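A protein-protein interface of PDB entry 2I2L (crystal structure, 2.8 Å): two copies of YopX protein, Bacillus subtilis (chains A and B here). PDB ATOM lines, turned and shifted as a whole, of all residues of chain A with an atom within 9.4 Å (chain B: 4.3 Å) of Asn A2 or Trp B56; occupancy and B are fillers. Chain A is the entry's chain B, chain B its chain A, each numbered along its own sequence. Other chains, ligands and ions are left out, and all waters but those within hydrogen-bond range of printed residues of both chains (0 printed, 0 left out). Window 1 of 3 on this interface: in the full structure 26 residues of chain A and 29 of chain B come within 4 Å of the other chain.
NE1 of Trp B56 lies within hydrogen-bond range of O of Asn A2. The backbone NH of Ile B25 lies within hydrogen-bond range of the backbone carbonyl oxygen of Leu A23 (3.1 Å). The backbone carbonyl oxygen (O) of Leu B23 sits at hydrogen-bond distance from the backbone NH (N) of Ile A25. The backbone carbonyl oxygen of Gly A91 sits at hydrogen-bond distance from the backbone NH of Phe B93 (2.9 Å).
The backbone NH (N) of Ala B58 is in hydrogen-bond range of the backbone carbonyl oxygen (O) of Ile B65 (3.0 Å). The side-chain hydroxyl of Tyr B5 sits at hydrogen-bond distance from the backbone NH of Leu B23 (3.5 Å).
O of Leu B54 touches ND2 of Asn A2, at 3.6 Å. Thr A3 touches Ile B25 (CG2 to CG2, 3.3 Å). Leu A23 touches Leu B23. CA of Ile A24 touches O of Leu B23, 3.5 Å away. CG2 of Ile A25 touches CE2 of Tyr B5 (3.6 Å). Trp B56 touches Ile A25. Trp B56 touches Trp A56. CA of Gly A91 touches CB of Ala B58 (3.5 Å).
Of chain A, only Asn A2 comes within 4 Å of Leu B54. No residue of chain A comes within 4 Å of Gly B57. Of the printed residues of chain A, Ala B58 touches Gly A91. Of the printed residues of chain B, Gly A91 touches Ala B58 (3.5 Å) and Phe B93 (2.9 Å). Printed residues of chain B within 4 Å of Trp A56: Trp B56 (3.3 Å). The nearest residue of chain A that does not touch Trp B56 is Thr A3 (4.8 Å).
Of the 12 printed residues of chain B, 7 touch a printed residue of chain A. Hydrophobic or aromatic side chains of chain B within 4 Å of the printed part of chain A: Tyr B5, Ile B25, Leu B54, Trp B56, Ala B58 and Phe B93. Among the printed residues, no Asp or Glu carboxylate lies within 4 Å of a Lys or Arg side-chain nitrogen of the other chain.
Leu A23 touches Ile B25, and with the chains exchanged Ile A25 touches Leu B23. Ile A25 touches Tyr B5, but with the chains exchanged Tyr A5 does not touch Ile B25 (4.04 Å). Ile A25 touches Trp B56, but with the chains exchanged Trp A56 does not touch Ile B25 (4.01 Å). Trp B56 touches its own counterpart, Trp A56. Of the 12 pairs that touch across the chains among the printed residues, 4 have their exchanged pair printed and touching as well.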
ATOM      1  N   MET A   1     -27.063  -2.420 -17.379  1.00  0.00           N
ATOM      2  CA  MET A   1     -25.905  -1.918 -16.581  1.00  0.00           C
ATOM      3  C   MET A   1     -25.844  -0.393 -16.597  1.00  0.00           C
ATOM      4  O   MET A   1     -25.419   0.217 -17.584  1.00  0.00           O
ATOM      5  CB  MET A   1     -24.585  -2.501 -17.119  1.00  0.00           C
ATOM      6  N   ASN A   2     -26.289   0.211 -15.498  1.00  0.00           N
ATOM      7  CA  ASN A   2     -26.274   1.664 -15.330  1.00  0.00           C
ATOM      8  C   ASN A   2     -24.809   2.038 -15.193  1.00  0.00           C
ATOM      9  O   ASN A   2     -24.310   2.236 -14.087  1.00  0.00           O
ATOM     10  CB  ASN A   2     -27.027   2.028 -14.052  1.00  0.00           C
ATOM     11  CG  ASN A   2     -26.885   0.958 -12.979  1.00  0.00           C
ATOM     12  OD1 ASN A   2     -25.781   0.641 -12.530  1.00  0.00           O
ATOM     13  ND2 ASN A   2     -28.010   0.389 -12.573  1.00  0.00           N
ATOM     14  N   THR A   3     -24.107   2.134 -16.310  1.00  0.00           N
ATOM     15  CA  THR A   3     -22.697   2.431 -16.202  1.00  0.00           C
ATOM     16  C   THR A   3     -22.070   3.197 -17.353  1.00  0.00           C
ATOM     17  O   THR A   3     -21.010   3.793 -17.189  1.00  0.00           O
ATOM     18  CB  THR A   3     -21.928   1.113 -15.936  1.00  0.00           C
ATOM     19  OG1 THR A   3     -21.793   0.936 -14.522  1.00  0.00           O
ATOM     20  CG2 THR A   3     -20.564   1.123 -16.588  1.00  0.00           C
ATOM     21  N   ALA A   4     -22.727   3.201 -18.507  1.00  0.00           N
ATOM     22  CA  ALA A   4     -22.197   3.902 -19.681  1.00  0.00           C
ATOM     23  C   ALA A   4     -21.868   5.373 -19.430  1.00  0.00           C
ATOM     24  O   ALA A   4     -22.665   6.126 -18.862  1.00  0.00           O
ATOM     25  CB  ALA A   4     -23.173   3.792 -20.855  1.00  0.00           C
ATOM     26  N   TYR A   5     -20.672   5.762 -19.856  1.00  0.00           N
ATOM     27  CA  TYR A   5     -20.219   7.140 -19.736  1.00  0.00           C
ATOM     28  C   TYR A   5     -19.084   7.328 -20.736  1.00  0.00           C
ATOM     29  O   TYR A   5     -18.576   6.353 -21.309  1.00  0.00           O
ATOM     30  CB  TYR A   5     -19.716   7.448 -18.312  1.00  0.00           C
ATOM     31  CG  TYR A   5     -18.373   6.848 -17.992  1.00  0.00           C
ATOM     32  CD1 TYR A   5     -18.276   5.579 -17.447  1.00  0.00           C
ATOM     33  CD2 TYR A   5     -17.190   7.513 -18.336  1.00  0.00           C
ATOM     34  CE1 TYR A   5     -17.038   4.968 -17.258  1.00  0.00           C
ATOM     35  CE2 TYR A   5     -15.952   6.919 -18.160  1.00  0.00           C
ATOM     36  CZ  TYR A   5     -15.881   5.638 -17.623  1.00  0.00           C
ATOM     37  OH  TYR A   5     -14.666   4.991 -17.494  1.00  0.00           O
ATOM     38  N   TRP A  16     -16.297   4.354 -21.813  1.00  0.00           N
ATOM     39  CA  TRP A  16     -16.197   3.403 -20.704  1.00  0.00           C
ATOM     40  C   TRP A  16     -15.681   2.014 -21.073  1.00  0.00           C
ATOM     41  O   TRP A  16     -14.941   1.390 -20.307  1.00  0.00           O
ATOM     42  CB  TRP A  16     -17.559   3.262 -20.017  1.00  0.00           C
ATOM     43  CG  TRP A  16     -18.608   2.691 -20.915  1.00  0.00           C
ATOM     44  CD1 TRP A  16     -19.385   3.370 -21.806  1.00  0.00           C
ATOM     45  CD2 TRP A  16     -18.937   1.306 -21.068  1.00  0.00           C
ATOM     46  NE1 TRP A  16     -20.174   2.492 -22.510  1.00  0.00           N
ATOM     47  CE2 TRP A  16     -19.917   1.214 -22.077  1.00  0.00           C
ATOM     48  CE3 TRP A  16     -18.490   0.125 -20.453  1.00  0.00           C
ATOM     49  CZ2 TRP A  16     -20.467  -0.012 -22.490  1.00  0.00           C
ATOM     50  CZ3 TRP A  16     -19.037  -1.100 -20.864  1.00  0.00           C
ATOM     51  CH2 TRP A  16     -20.013  -1.153 -21.873  1.00  0.00           C
ATOM     52  N   LEU A  23     -13.400   4.794 -14.228  1.00  0.00           N
ATOM     53  CA  LEU A  23     -13.872   6.088 -13.759  1.00  0.00           C
ATOM     54  C   LEU A  23     -13.975   6.077 -12.227  1.00  0.00           C
ATOM     55  O   LEU A  23     -14.553   5.162 -11.640  1.00  0.00           O
ATOM     56  CB  LEU A  23     -15.239   6.376 -14.364  1.00  0.00           C
ATOM     57  CG  LEU A  23     -15.768   7.783 -14.115  1.00  0.00           C
ATOM     58  CD1 LEU A  23     -14.830   8.802 -14.760  1.00  0.00           C
ATOM     59  CD2 LEU A  23     -17.180   7.895 -14.694  1.00  0.00           C
ATOM     60  N   ILE A  24     -13.422   7.092 -11.581  1.00  0.00           N
ATOM     61  CA  ILE A  24     -13.454   7.143 -10.124  1.00  0.00           C
ATOM     62  C   ILE A  24     -14.193   8.352  -9.573  1.00  0.00           C
ATOM     63  O   ILE A  24     -13.748   9.487  -9.735  1.00  0.00           O
ATOM     64  CB  ILE A  24     -12.011   7.170  -9.512  1.00  0.00           C
ATOM     65  CG1 ILE A  24     -11.093   6.206 -10.274  1.00  0.00           C
ATOM     66  CG2 ILE A  24     -12.066   6.830  -8.015  1.00  0.00           C
ATOM     67  CD1 ILE A  24     -11.614   4.772 -10.366  1.00  0.00           C
ATOM     68  N   ILE A  25     -15.302   8.101  -8.894  1.00  0.00           N
ATOM     69  CA  ILE A  25     -16.080   9.173  -8.293  1.00  0.00           C
ATOM     70  C   ILE A  25     -15.685   9.315  -6.818  1.00  0.00           C
ATOM     71  O   ILE A  25     -15.833   8.375  -6.035  1.00  0.00           O
ATOM     72  CB  ILE A  25     -17.588   8.869  -8.372  1.00  0.00           C
ATOM     73  CG1 ILE A  25     -18.064   8.948  -9.818  1.00  0.00           C
ATOM     74  CG2 ILE A  25     -18.352   9.845  -7.497  1.00  0.00           C
ATOM     75  CD1 ILE A  25     -19.456   8.459 -10.009  1.00  0.00           C
ATOM     76  N   TRP A  31     -14.369  13.524  -9.898  1.00  0.00           N
ATOM     77  CA  TRP A  31     -14.199  12.276 -10.611  1.00  0.00           C
ATOM     78  C   TRP A  31     -12.823  12.267 -11.244  1.00  0.00           C
ATOM     79  O   TRP A  31     -12.193  13.314 -11.392  1.00  0.00           O
ATOM     80  CB  TRP A  31     -15.279  12.100 -11.679  1.00  0.00           C
ATOM     81  CG  TRP A  31     -15.324  13.177 -12.713  1.00  0.00           C
ATOM     82  CD1 TRP A  31     -16.235  14.179 -12.801  1.00  0.00           C
ATOM     83  CD2 TRP A  31     -14.469  13.308 -13.852  1.00  0.00           C
ATOM     84  NE1 TRP A  31     -16.012  14.922 -13.927  1.00  0.00           N
ATOM     85  CE2 TRP A  31     -14.938  14.411 -14.594  1.00  0.00           C
ATOM     86  CE3 TRP A  31     -13.352  12.597 -14.321  1.00  0.00           C
ATOM     87  CZ2 TRP A  31     -14.337  14.826 -15.783  1.00  0.00           C
ATOM     88  CZ3 TRP A  31     -12.744  13.007 -15.512  1.00  0.00           C
ATOM     89  CH2 TRP A  31     -13.242  14.115 -16.232  1.00  0.00           C
ATOM     90  N   LEU A  54     -17.413  14.996 -18.033  1.00  0.00           N
ATOM     91  CA  LEU A  54     -17.982  13.669 -17.790  1.00  0.00           C
ATOM     92  C   LEU A  54     -19.418  13.649 -18.352  1.00  0.00           C
ATOM     93  O   LEU A  54     -20.262  14.444 -17.939  1.00  0.00           O
ATOM     94  CB  LEU A  54     -18.023  13.379 -16.280  1.00  0.00           C
ATOM     95  CG  LEU A  54     -17.929  11.932 -15.760  1.00  0.00           C
ATOM     96  CD1 LEU A  54     -18.312  11.894 -14.303  1.00  0.00           C
ATOM     97  CD2 LEU A  54     -18.840  11.009 -16.540  1.00  0.00           C
ATOM     98  N   TRP A  56     -22.738  11.101 -19.052  1.00  0.00           N
ATOM     99  CA  TRP A  56     -23.380   9.812 -18.841  1.00  0.00           C
ATOM    100  C   TRP A  56     -24.190   9.360 -20.045  1.00  0.00           C
ATOM    101  O   TRP A  56     -24.583  10.162 -20.908  1.00  0.00           O
ATOM    102  CB  TRP A  56     -24.306   9.860 -17.630  1.00  0.00           C
ATOM    103  CG  TRP A  56     -23.612  10.154 -16.355  1.00  0.00           C
ATOM    104  CD1 TRP A  56     -23.750  11.272 -15.596  1.00  0.00           C
ATOM    105  CD2 TRP A  56     -22.687   9.305 -15.660  1.00  0.00           C
ATOM    106  NE1 TRP A  56     -22.968  11.179 -14.468  1.00  0.00           N
ATOM    107  CE2 TRP A  56     -22.306   9.982 -14.483  1.00  0.00           C
ATOM    108  CE3 TRP A  56     -22.150   8.042 -15.915  1.00  0.00           C
ATOM    109  CZ2 TRP A  56     -21.411   9.434 -13.557  1.00  0.00           C
ATOM    110  CZ3 TRP A  56     -21.259   7.496 -14.989  1.00  0.00           C
ATOM    111  CH2 TRP A  56     -20.900   8.197 -13.826  1.00  0.00           C
ATOM    112  N   GLY A  57     -24.449   8.062 -20.092  1.00  0.00           N
ATOM    113  CA  GLY A  57     -25.230   7.535 -21.184  1.00  0.00           C
ATOM    114  C   GLY A  57     -26.516   6.919 -20.687  1.00  0.00           C
ATOM    115  O   GLY A  57     -26.614   6.526 -19.537  1.00  0.00           O
ATOM    116  N   ALA A  58     -27.507   6.856 -21.562  1.00  0.00           N
ATOM    117  CA  ALA A  58     -28.790   6.257 -21.249  1.00  0.00           C
ATOM    118  C   ALA A  58     -29.126   5.327 -22.415  1.00  0.00           C
ATOM    119  O   ALA A  58     -28.823   5.620 -23.572  1.00  0.00           O
ATOM    120  CB  ALA A  58     -29.868   7.339 -21.114  1.00  0.00           C
ATOM    121  N   LYS A  59     -29.731   4.190 -22.118  1.00  0.00           N
ATOM    122  CA  LYS A  59     -30.100   3.295 -23.186  1.00  0.00           C
ATOM    123  C   LYS A  59     -31.534   3.655 -23.602  1.00  0.00           C
ATOM    124  O   LYS A  59     -32.455   3.642 -22.786  1.00  0.00           O
ATOM    125  CB  LYS A  59     -30.019   1.849 -22.708  1.00  0.00           C
ATOM    126  CG  LYS A  59     -30.098   0.832 -23.835  1.00  0.00           C
ATOM    127  CD  LYS A  59     -30.047  -0.591 -23.304  1.00  0.00           C
ATOM    128  CE  LYS A  59     -30.016  -1.599 -24.431  1.00  0.00           C
ATOM    129  NZ  LYS A  59     -29.923  -2.972 -23.894  1.00  0.00           N
ATOM    130  N   PHE A  64     -27.292   3.419 -26.825  1.00  0.00           N
ATOM    131  CA  PHE A  64     -26.925   4.195 -25.643  1.00  0.00           C
ATOM    132  C   PHE A  64     -26.681   5.609 -26.165  1.00  0.00           C
ATOM    133  O   PHE A  64     -26.021   5.782 -27.186  1.00  0.00           O
ATOM    134  CB  PHE A  64     -25.642   3.653 -25.017  1.00  0.00           C
ATOM    135  CG  PHE A  64     -25.858   2.948 -23.716  1.00  0.00           C
ATOM    136  CD1 PHE A  64     -25.392   1.647 -23.527  1.00  0.00           C
ATOM    137  CD2 PHE A  64     -26.541   3.576 -22.678  1.00  0.00           C
ATOM    138  CE1 PHE A  64     -25.603   0.982 -22.321  1.00  0.00           C
ATOM    139  CE2 PHE A  64     -26.757   2.925 -21.470  1.00  0.00           C
ATOM    140  CZ  PHE A  64     -26.289   1.621 -21.288  1.00  0.00           C
ATOM    141  N   PHE A  88     -28.485  16.727 -20.653  1.00  0.00           N
ATOM    142  CA  PHE A  88     -29.024  15.938 -19.562  1.00  0.00           C
ATOM    143  C   PHE A  88     -29.240  16.905 -18.413  1.00  0.00           C
ATOM    144  O   PHE A  88     -28.298  17.269 -17.700  1.00  0.00           O
ATOM    145  CB  PHE A  88     -28.048  14.828 -19.177  1.00  0.00           C
ATOM    146  CG  PHE A  88     -28.495  14.004 -18.013  1.00  0.00           C
ATOM    147  CD1 PHE A  88     -29.817  13.592 -17.901  1.00  0.00           C
ATOM    148  CD2 PHE A  88     -27.592  13.628 -17.029  1.00  0.00           C
ATOM    149  CE1 PHE A  88     -30.239  12.822 -16.825  1.00  0.00           C
ATOM    150  CE2 PHE A  88     -28.004  12.860 -15.951  1.00  0.00           C
ATOM    151  CZ  PHE A  88     -29.337  12.457 -15.853  1.00  0.00           C
ATOM    152  N   GLY A  91     -33.008  15.522 -14.577  1.00  0.00           N
ATOM    153  CA  GLY A  91     -33.318  14.107 -14.523  1.00  0.00           C
ATOM    154  C   GLY A  91     -33.835  13.531 -15.820  1.00  0.00           C
ATOM    155  O   GLY A  91     -34.375  12.426 -15.851  1.00  0.00           O
ATOM    156  N   PHE A  93     -32.972  13.239 -20.221  1.00  0.00           N
ATOM    157  CA  PHE A  93     -32.169  13.470 -21.414  1.00  0.00           C
ATOM    158  C   PHE A  93     -33.131  14.119 -22.392  1.00  0.00           C
ATOM    159  O   PHE A  93     -33.764  13.441 -23.202  1.00  0.00           O
ATOM    160  CB  PHE A  93     -31.662  12.141 -21.982  1.00  0.00           C
ATOM    161  CG  PHE A  93     -30.448  11.616 -21.286  1.00  0.00           C
ATOM    162  CD1 PHE A  93     -29.200  11.681 -21.894  1.00  0.00           C
ATOM    163  CD2 PHE A  93     -30.536  11.097 -20.004  1.00  0.00           C
ATOM    164  CE1 PHE A  93     -28.050  11.241 -21.231  1.00  0.00           C
ATOM    165  CE2 PHE A  93     -29.390  10.657 -19.330  1.00  0.00           C
ATOM    166  CZ  PHE A  93     -28.145  10.729 -19.946  1.00  0.00           C
ATOM    167  N   ALA B   4     -23.913  12.453  -8.098  1.00  0.00           N
ATOM    168  CA  ALA B   4     -24.777  11.888  -7.057  1.00  0.00           C
ATOM    169  C   ALA B   4     -25.218  10.475  -7.369  1.00  0.00           C
ATOM    170  O   ALA B   4     -25.796  10.209  -8.419  1.00  0.00           O
ATOM    171  CB  ALA B   4     -25.995  12.765  -6.840  1.00  0.00           C
ATOM    172  N   TYR B   5     -24.941   9.574  -6.436  1.00  0.00           N
ATOM    173  CA  TYR B   5     -25.295   8.170  -6.590  1.00  0.00           C
ATOM    174  C   TYR B   5     -25.446   7.590  -5.188  1.00  0.00           C
ATOM    175  O   TYR B   5     -25.087   8.236  -4.197  1.00  0.00           O
ATOM    176  CB  TYR B   5     -24.170   7.418  -7.348  1.00  0.00           C
ATOM    177  CG  TYR B   5     -22.933   7.104  -6.513  1.00  0.00           C
ATOM    178  CD1 TYR B   5     -22.946   6.070  -5.563  1.00  0.00           C
ATOM    179  CD2 TYR B   5     -21.783   7.888  -6.607  1.00  0.00           C
ATOM    180  CE1 TYR B   5     -21.866   5.843  -4.732  1.00  0.00           C
ATOM    181  CE2 TYR B   5     -20.682   7.662  -5.770  1.00  0.00           C
ATOM    182  CZ  TYR B   5     -20.740   6.646  -4.837  1.00  0.00           C
ATOM    183  OH  TYR B   5     -19.686   6.471  -3.976  1.00  0.00           O
ATOM    184  N   LEU B  23     -16.764   5.584  -5.601  1.00  0.00           N
ATOM    185  CA  LEU B  23     -17.320   4.610  -6.518  1.00  0.00           C
ATOM    186  C   LEU B  23     -16.341   4.392  -7.668  1.00  0.00           C
ATOM    187  O   LEU B  23     -15.707   5.337  -8.156  1.00  0.00           O
ATOM    188  CB  LEU B  23     -18.652   5.119  -7.052  1.00  0.00           C
ATOM    189  CG  LEU B  23     -19.392   4.190  -8.001  1.00  0.00           C
ATOM    190  CD1 LEU B  23     -19.555   2.799  -7.359  1.00  0.00           C
ATOM    191  CD2 LEU B  23     -20.737   4.833  -8.343  1.00  0.00           C
ATOM    192  N   ILE B  25     -16.191   2.580 -11.414  1.00  0.00           N
ATOM    193  CA  ILE B  25     -16.811   1.884 -12.526  1.00  0.00           C
ATOM    194  C   ILE B  25     -15.696   1.327 -13.403  1.00  0.00           C
ATOM    195  O   ILE B  25     -14.769   2.058 -13.757  1.00  0.00           O
ATOM    196  CB  ILE B  25     -17.689   2.834 -13.346  1.00  0.00           C
ATOM    197  CG1 ILE B  25     -18.875   3.295 -12.498  1.00  0.00           C
ATOM    198  CG2 ILE B  25     -18.170   2.132 -14.612  1.00  0.00           C
ATOM    199  CD1 ILE B  25     -19.867   4.159 -13.249  1.00  0.00           C
ATOM    200  N   LEU B  54     -26.937  -0.146  -7.430  1.00  0.00           N
ATOM    201  CA  LEU B  54     -26.372   1.189  -7.641  1.00  0.00           C
ATOM    202  C   LEU B  54     -27.491   2.072  -8.247  1.00  0.00           C
ATOM    203  O   LEU B  54     -28.064   1.731  -9.285  1.00  0.00           O
ATOM    204  CB  LEU B  54     -25.183   1.127  -8.615  1.00  0.00           C
ATOM    205  CG  LEU B  54     -24.039   2.165  -8.543  1.00  0.00           C
ATOM    206  CD1 LEU B  54     -23.368   2.237  -9.909  1.00  0.00           C
ATOM    207  CD2 LEU B  54     -24.545   3.547  -8.148  1.00  0.00           C
ATOM    208  N   MET B  55     -27.805   3.185  -7.583  1.00  0.00           N
ATOM    209  CA  MET B  55     -28.832   4.120  -8.047  1.00  0.00           C
ATOM    210  C   MET B  55     -28.254   5.517  -8.261  1.00  0.00           C
ATOM    211  O   MET B  55     -27.562   6.065  -7.392  1.00  0.00           O
ATOM    212  CB  MET B  55     -29.958   4.217  -7.028  1.00  0.00           C
ATOM    213  CG  MET B  55     -30.790   2.957  -6.870  1.00  0.00           C
ATOM    214  SD  MET B  55     -31.121   2.597  -5.001  1.00  0.00           S
ATOM    215  CE  MET B  55     -32.837   3.416  -4.783  1.00  0.00           C
ATOM    216  N   TRP B  56     -28.536   6.106  -9.413  1.00  0.00           N
ATOM    217  CA  TRP B  56     -28.026   7.439  -9.677  1.00  0.00           C
ATOM    218  C   TRP B  56     -28.981   8.524  -9.190  1.00  0.00           C
ATOM    219  O   TRP B  56     -30.194   8.316  -9.040  1.00  0.00           O
ATOM    220  CB  TRP B  56     -27.745   7.636 -11.172  1.00  0.00           C
ATOM    221  CG  TRP B  56     -26.684   6.725 -11.712  1.00  0.00           C
ATOM    222  CD1 TRP B  56     -26.878   5.611 -12.475  1.00  0.00           C
ATOM    223  CD2 TRP B  56     -25.269   6.829 -11.509  1.00  0.00           C
ATOM    224  NE1 TRP B  56     -25.676   5.015 -12.756  1.00  0.00           N
ATOM    225  CE2 TRP B  56     -24.667   5.743 -12.173  1.00  0.00           C
ATOM    226  CE3 TRP B  56     -24.447   7.738 -10.825  1.00  0.00           C
ATOM    227  CZ2 TRP B  56     -23.285   5.530 -12.186  1.00  0.00           C
ATOM    228  CZ3 TRP B  56     -23.063   7.528 -10.835  1.00  0.00           C
ATOM    229  CH2 TRP B  56     -22.500   6.428 -11.514  1.00  0.00           C
ATOM    230  N   GLY B  57     -28.410   9.691  -8.933  1.00  0.00           N
ATOM    231  CA  GLY B  57     -29.215  10.797  -8.476  1.00  0.00           C
ATOM    232  C   GLY B  57     -29.375  11.843  -9.556  1.00  0.00           C
ATOM    233  O   GLY B  57     -28.457  12.113 -10.323  1.00  0.00           O
ATOM    234  N   ALA B  58     -30.563  12.415  -9.637  1.00  0.00           N
ATOM    235  CA  ALA B  58     -30.816  13.460 -10.605  1.00  0.00           C
ATOM    236  C   ALA B  58     -31.027  14.732  -9.801  1.00  0.00           C
ATOM    237  O   ALA B  58     -31.663  14.716  -8.745  1.00  0.00           O
ATOM    238  CB  ALA B  58     -32.074  13.144 -11.434  1.00  0.00           C
ATOM    239  N   ILE B  65     -32.948  13.031  -6.340  1.00  0.00           N
ATOM    240  CA  ILE B  65     -33.834  11.894  -6.112  1.00  0.00           C
ATOM    241  C   ILE B  65     -33.022  10.758  -6.705  1.00  0.00           C
ATOM    242  O   ILE B  65     -32.050  11.028  -7.409  1.00  0.00           O
ATOM    243  CB  ILE B  65     -35.196  12.040  -6.841  1.00  0.00           C
ATOM    244  CG1 ILE B  65     -34.982  12.621  -8.237  1.00  0.00           C
ATOM    245  CG2 ILE B  65     -36.169  12.879  -6.001  1.00  0.00           C
ATOM    246  CD1 ILE B  65     -34.355  11.653  -9.216  1.00  0.00           C
ATOM    247  N   TYR B  66     -33.390   9.507  -6.443  1.00  0.00           N
ATOM    248  CA  TYR B  66     -32.599   8.394  -6.962  1.00  0.00           C
ATOM    249  C   TYR B  66     -33.385   7.201  -7.542  1.00  0.00           C
ATOM    250  O   TYR B  66     -33.269   6.878  -8.718  1.00  0.00           O
ATOM    251  CB  TYR B  66     -31.653   7.877  -5.862  1.00  0.00           C
ATOM    252  CG  TYR B  66     -30.669   8.882  -5.270  1.00  0.00           C
ATOM    253  CD1 TYR B  66     -31.064   9.812  -4.298  1.00  0.00           C
ATOM    254  CD2 TYR B  66     -29.321   8.864  -5.652  1.00  0.00           C
ATOM    255  CE1 TYR B  66     -30.137  10.690  -3.719  1.00  0.00           C
ATOM    256  CE2 TYR B  66     -28.389   9.728  -5.087  1.00  0.00           C
ATOM    257  CZ  TYR B  66     -28.797  10.638  -4.124  1.00  0.00           C
ATOM    258  OH  TYR B  66     -27.849  11.484  -3.572  1.00  0.00           O
ATOM    259  N   PHE B  93     -35.911  10.014 -15.410  1.00  0.00           N
ATOM    260  CA  PHE B  93     -36.423   9.613 -14.106  1.00  0.00           C
ATOM    261  C   PHE B  93     -37.915   9.908 -14.203  1.00  0.00           C
ATOM    262  O   PHE B  93     -38.335  11.068 -14.256  1.00  0.00           O
ATOM    263  CB  PHE B  93     -35.778  10.437 -12.993  1.00  0.00           C
ATOM    264  CG  PHE B  93     -34.334  10.102 -12.755  1.00  0.00           C
ATOM    265  CD1 PHE B  93     -33.938   9.459 -11.580  1.00  0.00           C
ATOM    266  CD2 PHE B  93     -33.369  10.424 -13.697  1.00  0.00           C
ATOM    267  CE1 PHE B  93     -32.589   9.145 -11.343  1.00  0.00           C
ATOM    268  CE2 PHE B  93     -32.017  10.114 -13.476  1.00  0.00           C
ATOM    269  CZ  PHE B  93     -31.624   9.471 -12.290  1.00  0.00           C
